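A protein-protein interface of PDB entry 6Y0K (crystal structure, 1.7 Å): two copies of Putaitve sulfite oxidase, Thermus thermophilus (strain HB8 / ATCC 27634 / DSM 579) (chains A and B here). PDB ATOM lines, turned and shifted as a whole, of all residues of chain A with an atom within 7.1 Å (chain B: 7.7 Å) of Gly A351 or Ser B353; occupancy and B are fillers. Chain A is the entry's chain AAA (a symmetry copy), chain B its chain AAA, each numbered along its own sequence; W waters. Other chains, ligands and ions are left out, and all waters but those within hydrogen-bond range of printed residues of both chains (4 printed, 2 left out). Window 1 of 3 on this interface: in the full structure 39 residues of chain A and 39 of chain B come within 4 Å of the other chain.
Leu B356 touches Val A300 (CD2 to CG1, 3.8 Å).
Arg B345 touches Trp A347 (NH1 to CE3, 3.2 Å).
Trp A347 touches Ser B353.
Trp A347 touches Leu B356 (CH2 to CB, 3.8 Å).
Pro B355 touches Ala A349.
Pro B242 touches Val A350.
Phe B243 touches Val A350 (CE1 to CG1, 3.5 Å).
Gly A351 touches Pro B355.
Ser A353 touches Trp B347 (OG to NE1, 3.7 Å).
O of Gln A354 touches CA of Gly B351, at 3.4 Å.
N of Gly A351 lies within hydrogen-bond range of OD1 of Asp A348 (3.3 Å).
OD1 of Asp B348 sits at hydrogen-bond distance from N of Gly B351 (3.3 Å).
The backbone carbonyl oxygen of Pro B355 is in hydrogen-bond range of the backbone NH of Val B372 (3.0 Å).
The backbone NH of Val A300 lies within hydrogen-bond range of the backbone carbonyl oxygen of Trp A347.
OE1 of Glu B303 is in salt-bridge range of NH2 of Arg B345, 2.9 Å away.
The backbone carbonyl oxygen (O) of Ala A346 is in hydrogen-bond range of the side-chain hydroxyl (OG) of Ser A353, 2.8 Å away.
Trp A347 touches Ser B353, and with the chains exchanged Ser A353 touches Trp B347.
Trp A347 touches Gln B354, and with the chains exchanged Gln A354 touches Trp B347.
Gly A351 touches Ser B353, and with the chains exchanged Ser A353 touches Gly B351.
Gly A351 touches Gln B354, and with the chains exchanged Gln A354 touches Gly B351.
Positions printed for both chains: 267, 346, 347, 348, 350, 351, 352, 353 and 354.
Of the 18 pairs that touch across the chains among the printed residues, 8 have their exchanged pair printed and touching as well.
Of the 23 printed residues of chain B, 10 touch a printed residue of chain A.
Hydrophobic or aromatic side chains of chain B within 4 Å of the printed part of chain A: Pro B242, Phe B243, Trp B347, Pro B355, Leu B356 and Ile B360.
Among the printed residues, 18 pairs touch across the chains.
Gly A351 touches just these residues of chain B: Ser B353, Gln B354 and Pro B355.
Ser B353 touches just these residues of chain A: Trp A347 (3.7 Å) and Gly A351 (3.0 Å).
Printed residues of chain B within 4 Å of Ala A349: Pro B355 and Ile B360.
Of the printed residues of chain B, Val A300 touches Leu B356 (3.8 Å).
Of the printed residues of chain A, Leu B356 touches Val A300 and Trp A347.
Water W4 lies within hydrogen-bond range of the backbone carbonyl oxygen of Ala A349 and the backbone NH of Asp B357.
Water W1 bridges the backbone carbonyl oxygen of Asp A348 and the backbone NH of Leu B356.
Water W3 bridges O of Val B350 and O of Ser A353.
Water W2 lies within hydrogen-bond range of O of Val A350 (3.0 Å), O of Ser B353 (3.0 Å) and ND2 of Asn B370 (3.3 Å).
N of Ser B353 is in hydrogen-bond range of O of Gly A351.
The backbone carbonyl oxygen (O) of Gly B351 is in hydrogen-bond range of the backbone NH (N) of Ser A353, 3.0 Å away.
The backbone carbonyl oxygen (O) of Gln B354 lies within hydrogen-bond range of the indole nitrogen (NE1) of Trp A347 (2.9 Å).
NE1 of Trp B347 sits at hydrogen-bond distance from O of Gln A354, at 2.9 Å.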
ATOM      1  N   ILE A 267      10.195 -30.479  -0.516  1.00  0.00           N
ATOM      2  CA  ILE A 267      10.151 -29.061  -0.947  1.00  0.00           C
ATOM      3  C   ILE A 267       8.779 -28.475  -0.587  1.00  0.00           C
ATOM      4  O   ILE A 267       7.761 -29.156  -0.716  1.00  0.00           O
ATOM      5  CB  ILE A 267      10.523 -28.908  -2.429  1.00  0.00           C
ATOM      6  CG1 ILE A 267      10.706 -27.429  -2.769  1.00  0.00           C
ATOM      7  CG2 ILE A 267       9.538 -29.586  -3.360  1.00  0.00           C
ATOM      8  CD1 ILE A 267      11.372 -27.200  -4.091  1.00  0.00           C
ATOM      9  N   VAL A 297      20.429 -28.246  -2.723  1.00  0.00           N
ATOM     10  CA  VAL A 297      20.587 -27.272  -3.840  1.00  0.00           C
ATOM     11  C   VAL A 297      19.792 -26.031  -3.491  1.00  0.00           C
ATOM     12  O   VAL A 297      18.869 -26.067  -2.681  1.00  0.00           O
ATOM     13  CB  VAL A 297      20.138 -27.853  -5.190  1.00  0.00           C
ATOM     14  CG1 VAL A 297      20.959 -29.072  -5.576  1.00  0.00           C
ATOM     15  CG2 VAL A 297      18.661 -28.190  -5.210  1.00  0.00           C
ATOM     16  N   VAL A 300      15.188 -22.113  -6.968  1.00  0.00           N
ATOM     17  CA  VAL A 300      15.257 -21.268  -8.189  1.00  0.00           C
ATOM     18  C   VAL A 300      14.164 -20.207  -8.087  1.00  0.00           C
ATOM     19  O   VAL A 300      14.442 -19.039  -8.400  1.00  0.00           O
ATOM     20  CB  VAL A 300      15.171 -22.122  -9.455  1.00  0.00           C
ATOM     21  CG1 VAL A 300      14.831 -21.287 -10.676  1.00  0.00           C
ATOM     22  CG2 VAL A 300      16.462 -22.884  -9.669  1.00  0.00           C
ATOM     23  N   ALA A 346       7.076 -23.665  -4.616  1.00  0.00           N
ATOM     24  CA  ALA A 346       8.544 -23.576  -4.657  1.00  0.00           C
ATOM     25  C   ALA A 346       9.073 -24.463  -5.786  1.00  0.00           C
ATOM     26  O   ALA A 346       8.466 -25.499  -6.084  1.00  0.00           O
ATOM     27  CB  ALA A 346       9.112 -23.978  -3.314  1.00  0.00           C
ATOM     28  N   TRP A 347      10.207 -24.073  -6.361  1.00  0.00           N
ATOM     29  CA  TRP A 347      10.859 -24.785  -7.486  1.00  0.00           C
ATOM     30  C   TRP A 347      12.356 -24.703  -7.233  1.00  0.00           C
ATOM     31  O   TRP A 347      12.840 -23.585  -7.083  1.00  0.00           O
ATOM     32  CB  TRP A 347      10.457 -24.119  -8.793  1.00  0.00           C
ATOM     33  CG  TRP A 347      10.937 -24.740 -10.064  1.00  0.00           C
ATOM     34  CD1 TRP A 347      11.028 -26.064 -10.377  1.00  0.00           C
ATOM     35  CD2 TRP A 347      11.297 -24.025 -11.255  1.00  0.00           C
ATOM     36  NE1 TRP A 347      11.444 -26.219 -11.674  1.00  0.00           N
ATOM     37  CE2 TRP A 347      11.627 -24.982 -12.233  1.00  0.00           C
ATOM     38  CE3 TRP A 347      11.434 -22.669 -11.557  1.00  0.00           C
ATOM     39  CZ2 TRP A 347      12.034 -24.624 -13.519  1.00  0.00           C
ATOM     40  CZ3 TRP A 347      11.831 -22.316 -12.829  1.00  0.00           C
ATOM     41  CH2 TRP A 347      12.121 -23.282 -13.792  1.00  0.00           C
ATOM     42  N   ASP A 348      13.066 -25.834  -7.178  1.00  0.00           N
ATOM     43  CA  ASP A 348      14.508 -25.790  -6.832  1.00  0.00           C
ATOM     44  C   ASP A 348      15.357 -26.155  -8.049  1.00  0.00           C
ATOM     45  O   ASP A 348      14.824 -26.469  -9.139  1.00  0.00           O
ATOM     46  CB  ASP A 348      14.847 -26.604  -5.579  1.00  0.00           C
ATOM     47  CG  ASP A 348      14.929 -28.099  -5.769  1.00  0.00           C
ATOM     48  OD1 ASP A 348      14.906 -28.552  -6.932  1.00  0.00           O
ATOM     49  OD2 ASP A 348      15.046 -28.796  -4.718  1.00  0.00           O
ATOM     50  N   ALA A 349      16.664 -26.091  -7.860  1.00  0.00           N
ATOM     51  CA  ALA A 349      17.644 -26.144  -8.968  1.00  0.00           C
ATOM     52  C   ALA A 349      17.669 -27.519  -9.631  1.00  0.00           C
ATOM     53  O   ALA A 349      18.158 -27.592 -10.766  1.00  0.00           O
ATOM     54  CB  ALA A 349      18.997 -25.758  -8.431  1.00  0.00           C
ATOM     55  N   VAL A 350      17.213 -28.592  -8.961  1.00  0.00           N
ATOM     56  CA  VAL A 350      17.155 -29.933  -9.627  1.00  0.00           C
ATOM     57  C   VAL A 350      15.758 -30.180 -10.192  1.00  0.00           C
ATOM     58  O   VAL A 350      15.489 -31.291 -10.651  1.00  0.00           O
ATOM     59  CB  VAL A 350      17.625 -31.087  -8.724  1.00  0.00           C
ATOM     60  CG1 VAL A 350      19.097 -30.938  -8.395  1.00  0.00           C
ATOM     61  CG2 VAL A 350      16.795 -31.235  -7.461  1.00  0.00           C
ATOM     62  N   GLY A 351      14.877 -29.191 -10.139  1.00  0.00           N
ATOM     63  CA  GLY A 351      13.565 -29.314 -10.788  1.00  0.00           C
ATOM     64  C   GLY A 351      12.485 -29.774  -9.830  1.00  0.00           C
ATOM     65  O   GLY A 351      11.364 -29.937 -10.281  1.00  0.00           O
ATOM     66  N   ARG A 352      12.783 -29.958  -8.549  1.00  0.00           N
ATOM     67  CA  ARG A 352      11.735 -30.400  -7.597  1.00  0.00           C
ATOM     68  C   ARG A 352      10.713 -29.282  -7.448  1.00  0.00           C
ATOM     69  O   ARG A 352      11.103 -28.086  -7.401  1.00  0.00           O
ATOM     70  CB  ARG A 352      12.314 -30.807  -6.251  1.00  0.00           C
ATOM     71  CG  ARG A 352      13.105 -32.094  -6.352  1.00  0.00           C
ATOM     72  CD  ARG A 352      13.720 -32.515  -5.046  1.00  0.00           C
ATOM     73  NE  ARG A 352      14.710 -31.589  -4.569  1.00  0.00           N
ATOM     74  CZ  ARG A 352      15.502 -31.790  -3.519  1.00  0.00           C
ATOM     75  NH1 ARG A 352      15.464 -32.933  -2.852  1.00  0.00           N
ATOM     76  NH2 ARG A 352      16.342 -30.850  -3.150  1.00  0.00           N
ATOM     77  N   SER A 353       9.457 -29.668  -7.313  1.00  0.00           N
ATOM     78  CA  SER A 353       8.367 -28.729  -6.984  1.00  0.00           C
ATOM     79  C   SER A 353       7.329 -29.478  -6.161  1.00  0.00           C
ATOM     80  O   SER A 353       7.584 -30.638  -5.732  1.00  0.00           O
ATOM     81  CB  SER A 353       7.809 -28.076  -8.227  1.00  0.00           C
ATOM     82  OG  SER A 353       6.985 -26.955  -7.896  1.00  0.00           O
ATOM     83  N   GLN A 354       6.209 -28.825  -5.948  1.00  0.00           N
ATOM     84  CA  GLN A 354       5.122 -29.296  -5.063  1.00  0.00           C
ATOM     85  C   GLN A 354       3.970 -29.792  -5.916  1.00  0.00           C
ATOM     86  O   GLN A 354       3.703 -29.269  -6.991  1.00  0.00           O
ATOM     87  CB  GLN A 354       4.649 -28.139  -4.189  1.00  0.00           C
ATOM     88  CG  GLN A 354       5.683 -27.632  -3.204  1.00  0.00           C
ATOM     89  CD  GLN A 354       5.175 -26.406  -2.495  1.00  0.00           C
ATOM     90  OE1 GLN A 354       5.666 -25.303  -2.728  1.00  0.00           O
ATOM     91  NE2 GLN A 354       4.187 -26.597  -1.622  1.00  0.00           N
ATOM     92  N   PRO B 242      16.111 -36.273  -7.301  1.00  0.00           N
ATOM     93  CA  PRO B 242      16.245 -36.950  -8.592  1.00  0.00           C
ATOM     94  C   PRO B 242      17.666 -37.450  -8.899  1.00  0.00           C
ATOM     95  O   PRO B 242      17.815 -38.447  -9.573  1.00  0.00           O
ATOM     96  CB  PRO B 242      15.826 -35.879  -9.602  1.00  0.00           C
ATOM     97  CG  PRO B 242      14.983 -34.925  -8.825  1.00  0.00           C
ATOM     98  CD  PRO B 242      15.479 -34.950  -7.400  1.00  0.00           C
ATOM     99  N   PHE B 243      18.670 -36.740  -8.403  1.00  0.00           N
ATOM    100  CA  PHE B 243      20.093 -37.145  -8.500  1.00  0.00           C
ATOM    101  C   PHE B 243      20.850 -36.329  -7.460  1.00  0.00           C
ATOM    102  O   PHE B 243      20.340 -35.296  -7.002  1.00  0.00           O
ATOM    103  CB  PHE B 243      20.600 -36.906  -9.930  1.00  0.00           C
ATOM    104  CG  PHE B 243      20.294 -35.523 -10.440  1.00  0.00           C
ATOM    105  CD1 PHE B 243      21.103 -34.442 -10.127  1.00  0.00           C
ATOM    106  CD2 PHE B 243      19.166 -35.293 -11.213  1.00  0.00           C
ATOM    107  CE1 PHE B 243      20.786 -33.168 -10.576  1.00  0.00           C
ATOM    108  CE2 PHE B 243      18.832 -34.016 -11.628  1.00  0.00           C
ATOM    109  CZ  PHE B 243      19.645 -32.956 -11.321  1.00  0.00           C
ATOM    110  N   ALA B 266      12.751 -39.097 -17.327  1.00  0.00           N
ATOM    111  CA  ALA B 266      12.771 -37.789 -16.651  1.00  0.00           C
ATOM    112  C   ALA B 266      11.710 -36.879 -17.286  1.00  0.00           C
ATOM    113  O   ALA B 266      11.591 -36.845 -18.515  1.00  0.00           O
ATOM    114  CB  ALA B 266      14.148 -37.171 -16.727  1.00  0.00           C
ATOM    115  N   ILE B 267      10.977 -36.160 -16.454  1.00  0.00           N
ATOM    116  CA  ILE B 267       9.936 -35.214 -16.919  1.00  0.00           C
ATOM    117  C   ILE B 267      10.575 -34.206 -17.883  1.00  0.00           C
ATOM    118  O   ILE B 267      11.706 -33.768 -17.662  1.00  0.00           O
ATOM    119  CB  ILE B 267       9.195 -34.563 -15.741  1.00  0.00           C
ATOM    120  CG1 ILE B 267       7.979 -33.793 -16.254  1.00  0.00           C
ATOM    121  CG2 ILE B 267      10.094 -33.697 -14.882  1.00  0.00           C
ATOM    122  CD1 ILE B 267       7.025 -33.396 -15.170  1.00  0.00           C
ATOM    123  N   ASN B 268       9.882 -33.872 -18.957  1.00  0.00           N
ATOM    124  CA  ASN B 268      10.509 -33.041 -20.012  1.00  0.00           C
ATOM    125  C   ASN B 268       9.448 -32.341 -20.848  1.00  0.00           C
ATOM    126  O   ASN B 268       8.297 -32.772 -20.851  1.00  0.00           O
ATOM    127  CB  ASN B 268      11.418 -33.898 -20.889  1.00  0.00           C
ATOM    128  CG  ASN B 268      12.679 -33.209 -21.349  1.00  0.00           C
ATOM    129  OD1 ASN B 268      12.698 -31.995 -21.519  1.00  0.00           O
ATOM    130  ND2 ASN B 268      13.738 -34.002 -21.555  1.00  0.00           N
ATOM    131  N   SER B 301       0.520 -29.337 -15.669  1.00  0.00           N
ATOM    132  CA  SER B 301       0.643 -28.191 -16.600  1.00  0.00           C
ATOM    133  C   SER B 301       1.885 -28.329 -17.460  1.00  0.00           C
ATOM    134  O   SER B 301       2.868 -28.941 -17.014  1.00  0.00           O
ATOM    135  CB  SER B 301       0.675 -26.888 -15.848  1.00  0.00           C
ATOM    136  OG  SER B 301       1.916 -26.709 -15.175  1.00  0.00           O
ATOM    137  N   GLU B 303       4.004 -25.012 -19.008  1.00  0.00           N
ATOM    138  CA  GLU B 303       3.974 -23.539 -18.850  1.00  0.00           C
ATOM    139  C   GLU B 303       5.099 -22.972 -19.697  1.00  0.00           C
ATOM    140  O   GLU B 303       6.106 -23.664 -19.924  1.00  0.00           O
ATOM    141  CB  GLU B 303       4.054 -23.148 -17.377  1.00  0.00           C
ATOM    142  CG  GLU B 303       2.937 -23.754 -16.544  1.00  0.00           C
ATOM    143  CD  GLU B 303       3.173 -23.654 -15.050  1.00  0.00           C
ATOM    144  OE1 GLU B 303       4.148 -22.990 -14.680  1.00  0.00           O
ATOM    145  OE2 GLU B 303       2.379 -24.234 -14.263  1.00  0.00           O
ATOM    146  N   ALA B 344      10.017 -23.513 -21.925  1.00  0.00           N
ATOM    147  CA  ALA B 344       8.874 -24.373 -21.576  1.00  0.00           C
ATOM    148  C   ALA B 344       9.244 -25.251 -20.380  1.00  0.00           C
ATOM    149  O   ALA B 344      10.402 -25.706 -20.312  1.00  0.00           O
ATOM    150  CB  ALA B 344       8.476 -25.184 -22.779  1.00  0.00           C
ATOM    151  N   ARG B 345       8.304 -25.460 -19.463  1.00  0.00           N
ATOM    152  CA  ARG B 345       8.521 -26.384 -18.321  1.00  0.00           C
ATOM    153  C   ARG B 345       7.264 -27.213 -18.090  1.00  0.00           C
ATOM    154  O   ARG B 345       6.151 -26.663 -18.121  1.00  0.00           O
ATOM    155  CB  ARG B 345       8.991 -25.618 -17.088  1.00  0.00           C
ATOM    156  CG  ARG B 345       7.904 -24.913 -16.311  1.00  0.00           C
ATOM    157  CD  ARG B 345       8.426 -24.398 -14.993  1.00  0.00           C
ATOM    158  NE  ARG B 345       7.355 -23.563 -14.485  1.00  0.00           N
ATOM    159  CZ  ARG B 345       7.489 -22.611 -13.587  1.00  0.00           C
ATOM    160  NH1 ARG B 345       8.663 -22.341 -13.054  1.00  0.00           N
ATOM    161  NH2 ARG B 345       6.428 -21.921 -13.230  1.00  0.00           N
ATOM    162  N   ALA B 346       7.453 -28.503 -17.838  1.00  0.00           N
ATOM    163  CA  ALA B 346       6.371 -29.433 -17.479  1.00  0.00           C
ATOM    164  C   ALA B 346       6.318 -29.583 -15.957  1.00  0.00           C
ATOM    165  O   ALA B 346       7.361 -29.498 -15.299  1.00  0.00           O
ATOM    166  CB  ALA B 346       6.597 -30.761 -18.166  1.00  0.00           C
ATOM    167  N   TRP B 347       5.125 -29.844 -15.431  1.00  0.00           N
ATOM    168  CA  TRP B 347       4.869 -29.996 -13.978  1.00  0.00           C
ATOM    169  C   TRP B 347       3.848 -31.113 -13.839  1.00  0.00           C
ATOM    170  O   TRP B 347       2.794 -30.992 -14.458  1.00  0.00           O
ATOM    171  CB  TRP B 347       4.358 -28.675 -13.425  1.00  0.00           C
ATOM    172  CG  TRP B 347       4.122 -28.585 -11.952  1.00  0.00           C
ATOM    173  CD1 TRP B 347       4.877 -29.102 -10.941  1.00  0.00           C
ATOM    174  CD2 TRP B 347       3.083 -27.820 -11.322  1.00  0.00           C
ATOM    175  NE1 TRP B 347       4.362 -28.732  -9.726  1.00  0.00           N
ATOM    176  CE2 TRP B 347       3.254 -27.953  -9.931  1.00  0.00           C
ATOM    177  CE3 TRP B 347       1.993 -27.099 -11.807  1.00  0.00           C
ATOM    178  CZ2 TRP B 347       2.400 -27.339  -9.013  1.00  0.00           C
ATOM    179  CZ3 TRP B 347       1.153 -26.487 -10.901  1.00  0.00           C
ATOM    180  CH2 TRP B 347       1.360 -26.606  -9.528  1.00  0.00           C
ATOM    181  N   ASP B 348       4.139 -32.165 -13.067  1.00  0.00           N
ATOM    182  CA  ASP B 348       3.205 -33.315 -12.993  1.00  0.00           C
ATOM    183  C   ASP B 348       2.555 -33.383 -11.612  1.00  0.00           C
ATOM    184  O   ASP B 348       2.856 -32.561 -10.714  1.00  0.00           O
ATOM    185  CB  ASP B 348       3.845 -34.634 -13.438  1.00  0.00           C
ATOM    186  CG  ASP B 348       4.753 -35.296 -12.430  1.00  0.00           C
ATOM    187  OD1 ASP B 348       4.777 -34.845 -11.267  1.00  0.00           O
ATOM    188  OD2 ASP B 348       5.416 -36.295 -12.839  1.00  0.00           O
ATOM    189  N   VAL B 350       2.694 -35.292  -9.053  1.00  0.00           N
ATOM    190  CA  VAL B 350       3.472 -35.520  -7.792  1.00  0.00           C
ATOM    191  C   VAL B 350       4.456 -34.374  -7.569  1.00  0.00           C
ATOM    192  O   VAL B 350       5.278 -34.465  -6.654  1.00  0.00           O
ATOM    193  CB  VAL B 350       4.163 -36.893  -7.737  1.00  0.00           C
ATOM    194  CG1 VAL B 350       3.133 -38.005  -7.702  1.00  0.00           C
ATOM    195  CG2 VAL B 350       5.159 -37.108  -8.863  1.00  0.00           C
ATOM    196  N   GLY B 351       4.407 -33.334  -8.390  1.00  0.00           N
ATOM    197  CA  GLY B 351       5.227 -32.140  -8.147  1.00  0.00           C
ATOM    198  C   GLY B 351       6.529 -32.164  -8.921  1.00  0.00           C
ATOM    199  O   GLY B 351       7.295 -31.229  -8.763  1.00  0.00           O
ATOM    200  N   ARG B 352       6.777 -33.171  -9.751  1.00  0.00           N
ATOM    201  CA  ARG B 352       8.043 -33.204 -10.524  1.00  0.00           C
ATOM    202  C   ARG B 352       8.028 -32.061 -11.529  1.00  0.00           C
ATOM    203  O   ARG B 352       6.960 -31.782 -12.135  1.00  0.00           O
ATOM    204  CB  ARG B 352       8.266 -34.544 -11.207  1.00  0.00           C
ATOM    205  CG  ARG B 352       8.569 -35.637 -10.203  1.00  0.00           C
ATOM    206  CD  ARG B 352       8.766 -36.986 -10.839  1.00  0.00           C
ATOM    207  NE  ARG B 352       7.578 -37.482 -11.479  1.00  0.00           N
ATOM    208  CZ  ARG B 352       7.439 -38.702 -11.991  1.00  0.00           C
ATOM    209  NH1 ARG B 352       8.412 -39.596 -11.885  1.00  0.00           N
ATOM    210  NH2 ARG B 352       6.318 -39.030 -12.591  1.00  0.00           N
ATOM    211  N   SER B 353       9.189 -31.470 -11.742  1.00  0.00           N
ATOM    212  CA  SER B 353       9.387 -30.467 -12.808  1.00  0.00           C
ATOM    213  C   SER B 353      10.822 -30.581 -13.303  1.00  0.00           C
ATOM    214  O   SER B 353      11.543 -31.547 -12.926  1.00  0.00           O
ATOM    215  CB  SER B 353       9.010 -29.082 -12.336  1.00  0.00           C
ATOM    216  OG  SER B 353       8.903 -28.174 -13.436  1.00  0.00           O
ATOM    217  N   GLN B 354      11.206 -29.629 -14.124  1.00  0.00           N
ATOM    218  CA  GLN B 354      12.501 -29.612 -14.837  1.00  0.00           C
ATOM    219  C   GLN B 354      13.411 -28.591 -14.183  1.00  0.00           C
ATOM    220  O   GLN B 354      12.965 -27.559 -13.698  1.00  0.00           O
ATOM    221  CB  GLN B 354      12.267 -29.230 -16.295  1.00  0.00           C
ATOM    222  CG  GLN B 354      11.464 -30.241 -17.089  1.00  0.00           C
ATOM    223  CD  GLN B 354      11.166 -29.708 -18.464  1.00  0.00           C
ATOM    224  OE1 GLN B 354      10.019 -29.385 -18.771  1.00  0.00           O
ATOM    225  NE2 GLN B 354      12.199 -29.619 -19.299  1.00  0.00           N
ATOM    226  N   PRO B 355      14.731 -28.836 -14.163  1.00  0.00           N
ATOM    227  CA  PRO B 355      15.658 -27.843 -13.644  1.00  0.00           C
ATOM    228  C   PRO B 355      15.758 -26.688 -14.645  1.00  0.00           C
ATOM    229  O   PRO B 355      15.824 -26.983 -15.835  1.00  0.00           O
ATOM    230  CB  PRO B 355      16.994 -28.581 -13.577  1.00  0.00           C
ATOM    231  CG  PRO B 355      16.876 -29.656 -14.608  1.00  0.00           C
ATOM    232  CD  PRO B 355      15.406 -30.043 -14.652  1.00  0.00           C
ATOM    233  N   LEU B 356      15.851 -25.453 -14.157  1.00  0.00           N
ATOM    234  CA  LEU B 356      16.009 -24.274 -15.050  1.00  0.00           C
ATOM    235  C   LEU B 356      17.353 -24.377 -15.774  1.00  0.00           C
ATOM    236  O   LEU B 356      17.411 -24.007 -16.961  1.00  0.00           O
ATOM    237  CB  LEU B 356      15.929 -22.984 -14.237  1.00  0.00           C
ATOM    238  CG  LEU B 356      16.081 -21.705 -15.058  1.00  0.00           C
ATOM    239  CD1 LEU B 356      15.004 -21.616 -16.129  1.00  0.00           C
ATOM    240  CD2 LEU B 356      16.029 -20.487 -14.152  1.00  0.00           C
ATOM    241  N   ASP B 357      18.391 -24.849 -15.086  1.00  0.00           N
ATOM    242  CA  ASP B 357      19.734 -25.062 -15.688  1.00  0.00           C
ATOM    243  C   ASP B 357      20.002 -26.565 -15.730  1.00  0.00           C
ATOM    244  O   ASP B 357      20.350 -27.147 -14.683  1.00  0.00           O
ATOM    245  CB  ASP B 357      20.817 -24.301 -14.926  1.00  0.00           C
ATOM    246  CG  ASP B 357      22.209 -24.443 -15.543  1.00  0.00           C
ATOM    247  OD1 ASP B 357      22.365 -25.200 -16.512  1.00  0.00           O
ATOM    248  OD2 ASP B 357      23.128 -23.764 -15.053  1.00  0.00           O
ATOM    249  N   ILE B 360      23.041 -28.654 -14.051  1.00  0.00           N
ATOM    250  CA  ILE B 360      23.186 -29.049 -12.625  1.00  0.00           C
ATOM    251  C   ILE B 360      23.291 -30.584 -12.552  1.00  0.00           C
ATOM    252  O   ILE B 360      23.922 -31.088 -11.601  1.00  0.00           O
ATOM    253  CB  ILE B 360      22.036 -28.500 -11.765  1.00  0.00           C
ATOM    254  CG1 ILE B 360      22.401 -28.616 -10.283  1.00  0.00           C
ATOM    255  CG2 ILE B 360      20.719 -29.192 -12.125  1.00  0.00           C
ATOM    256  CD1 ILE B 360      21.643 -27.718  -9.357  1.00  0.00           C
ATOM    257  N   ASN B 370      17.376 -32.946 -18.795  1.00  0.00           N
ATOM    258  CA  ASN B 370      15.968 -32.496 -18.929  1.00  0.00           C
ATOM    259  C   ASN B 370      15.840 -31.020 -18.590  1.00  0.00           C
ATOM    260  O   ASN B 370      14.759 -30.606 -18.152  1.00  0.00           O
ATOM    261  CB  ASN B 370      15.035 -33.397 -18.114  1.00  0.00           C
ATOM    262  CG  ASN B 370      15.128 -33.177 -16.629  1.00  0.00           C
ATOM    263  OD1 ASN B 370      16.164 -32.719 -16.131  1.00  0.00           O
ATOM    264  ND2 ASN B 370      14.052 -33.510 -15.924  1.00  0.00           N
ATOM    265  N   VAL B 372      15.202 -27.050 -18.766  1.00  0.00           N
ATOM    266  CA  VAL B 372      14.202 -26.181 -19.438  1.00  0.00           C
ATOM    267  C   VAL B 372      14.737 -25.829 -20.822  1.00  0.00           C
ATOM    268  O   VAL B 372      15.854 -25.306 -20.916  1.00  0.00           O
ATOM    269  CB  VAL B 372      13.900 -24.957 -18.567  1.00  0.00           C
ATOM    270  CG1 VAL B 372      13.193 -23.847 -19.323  1.00  0.00           C
ATOM    271  CG2 VAL B 372      13.060 -25.367 -17.378  1.00  0.00           C
HETATM  272  O   HOH W   1      14.760 -25.047 -11.536  1.00  0.00           O
HETATM  273  O   HOH W   2      14.150 -32.964 -12.698  1.00  0.00           O
HETATM  274  O   HOH W   3       6.808 -33.208  -4.449  1.00  0.00           O
HETATM  275  O   HOH W   4      18.972 -25.664 -12.353  1.00  0.00           O
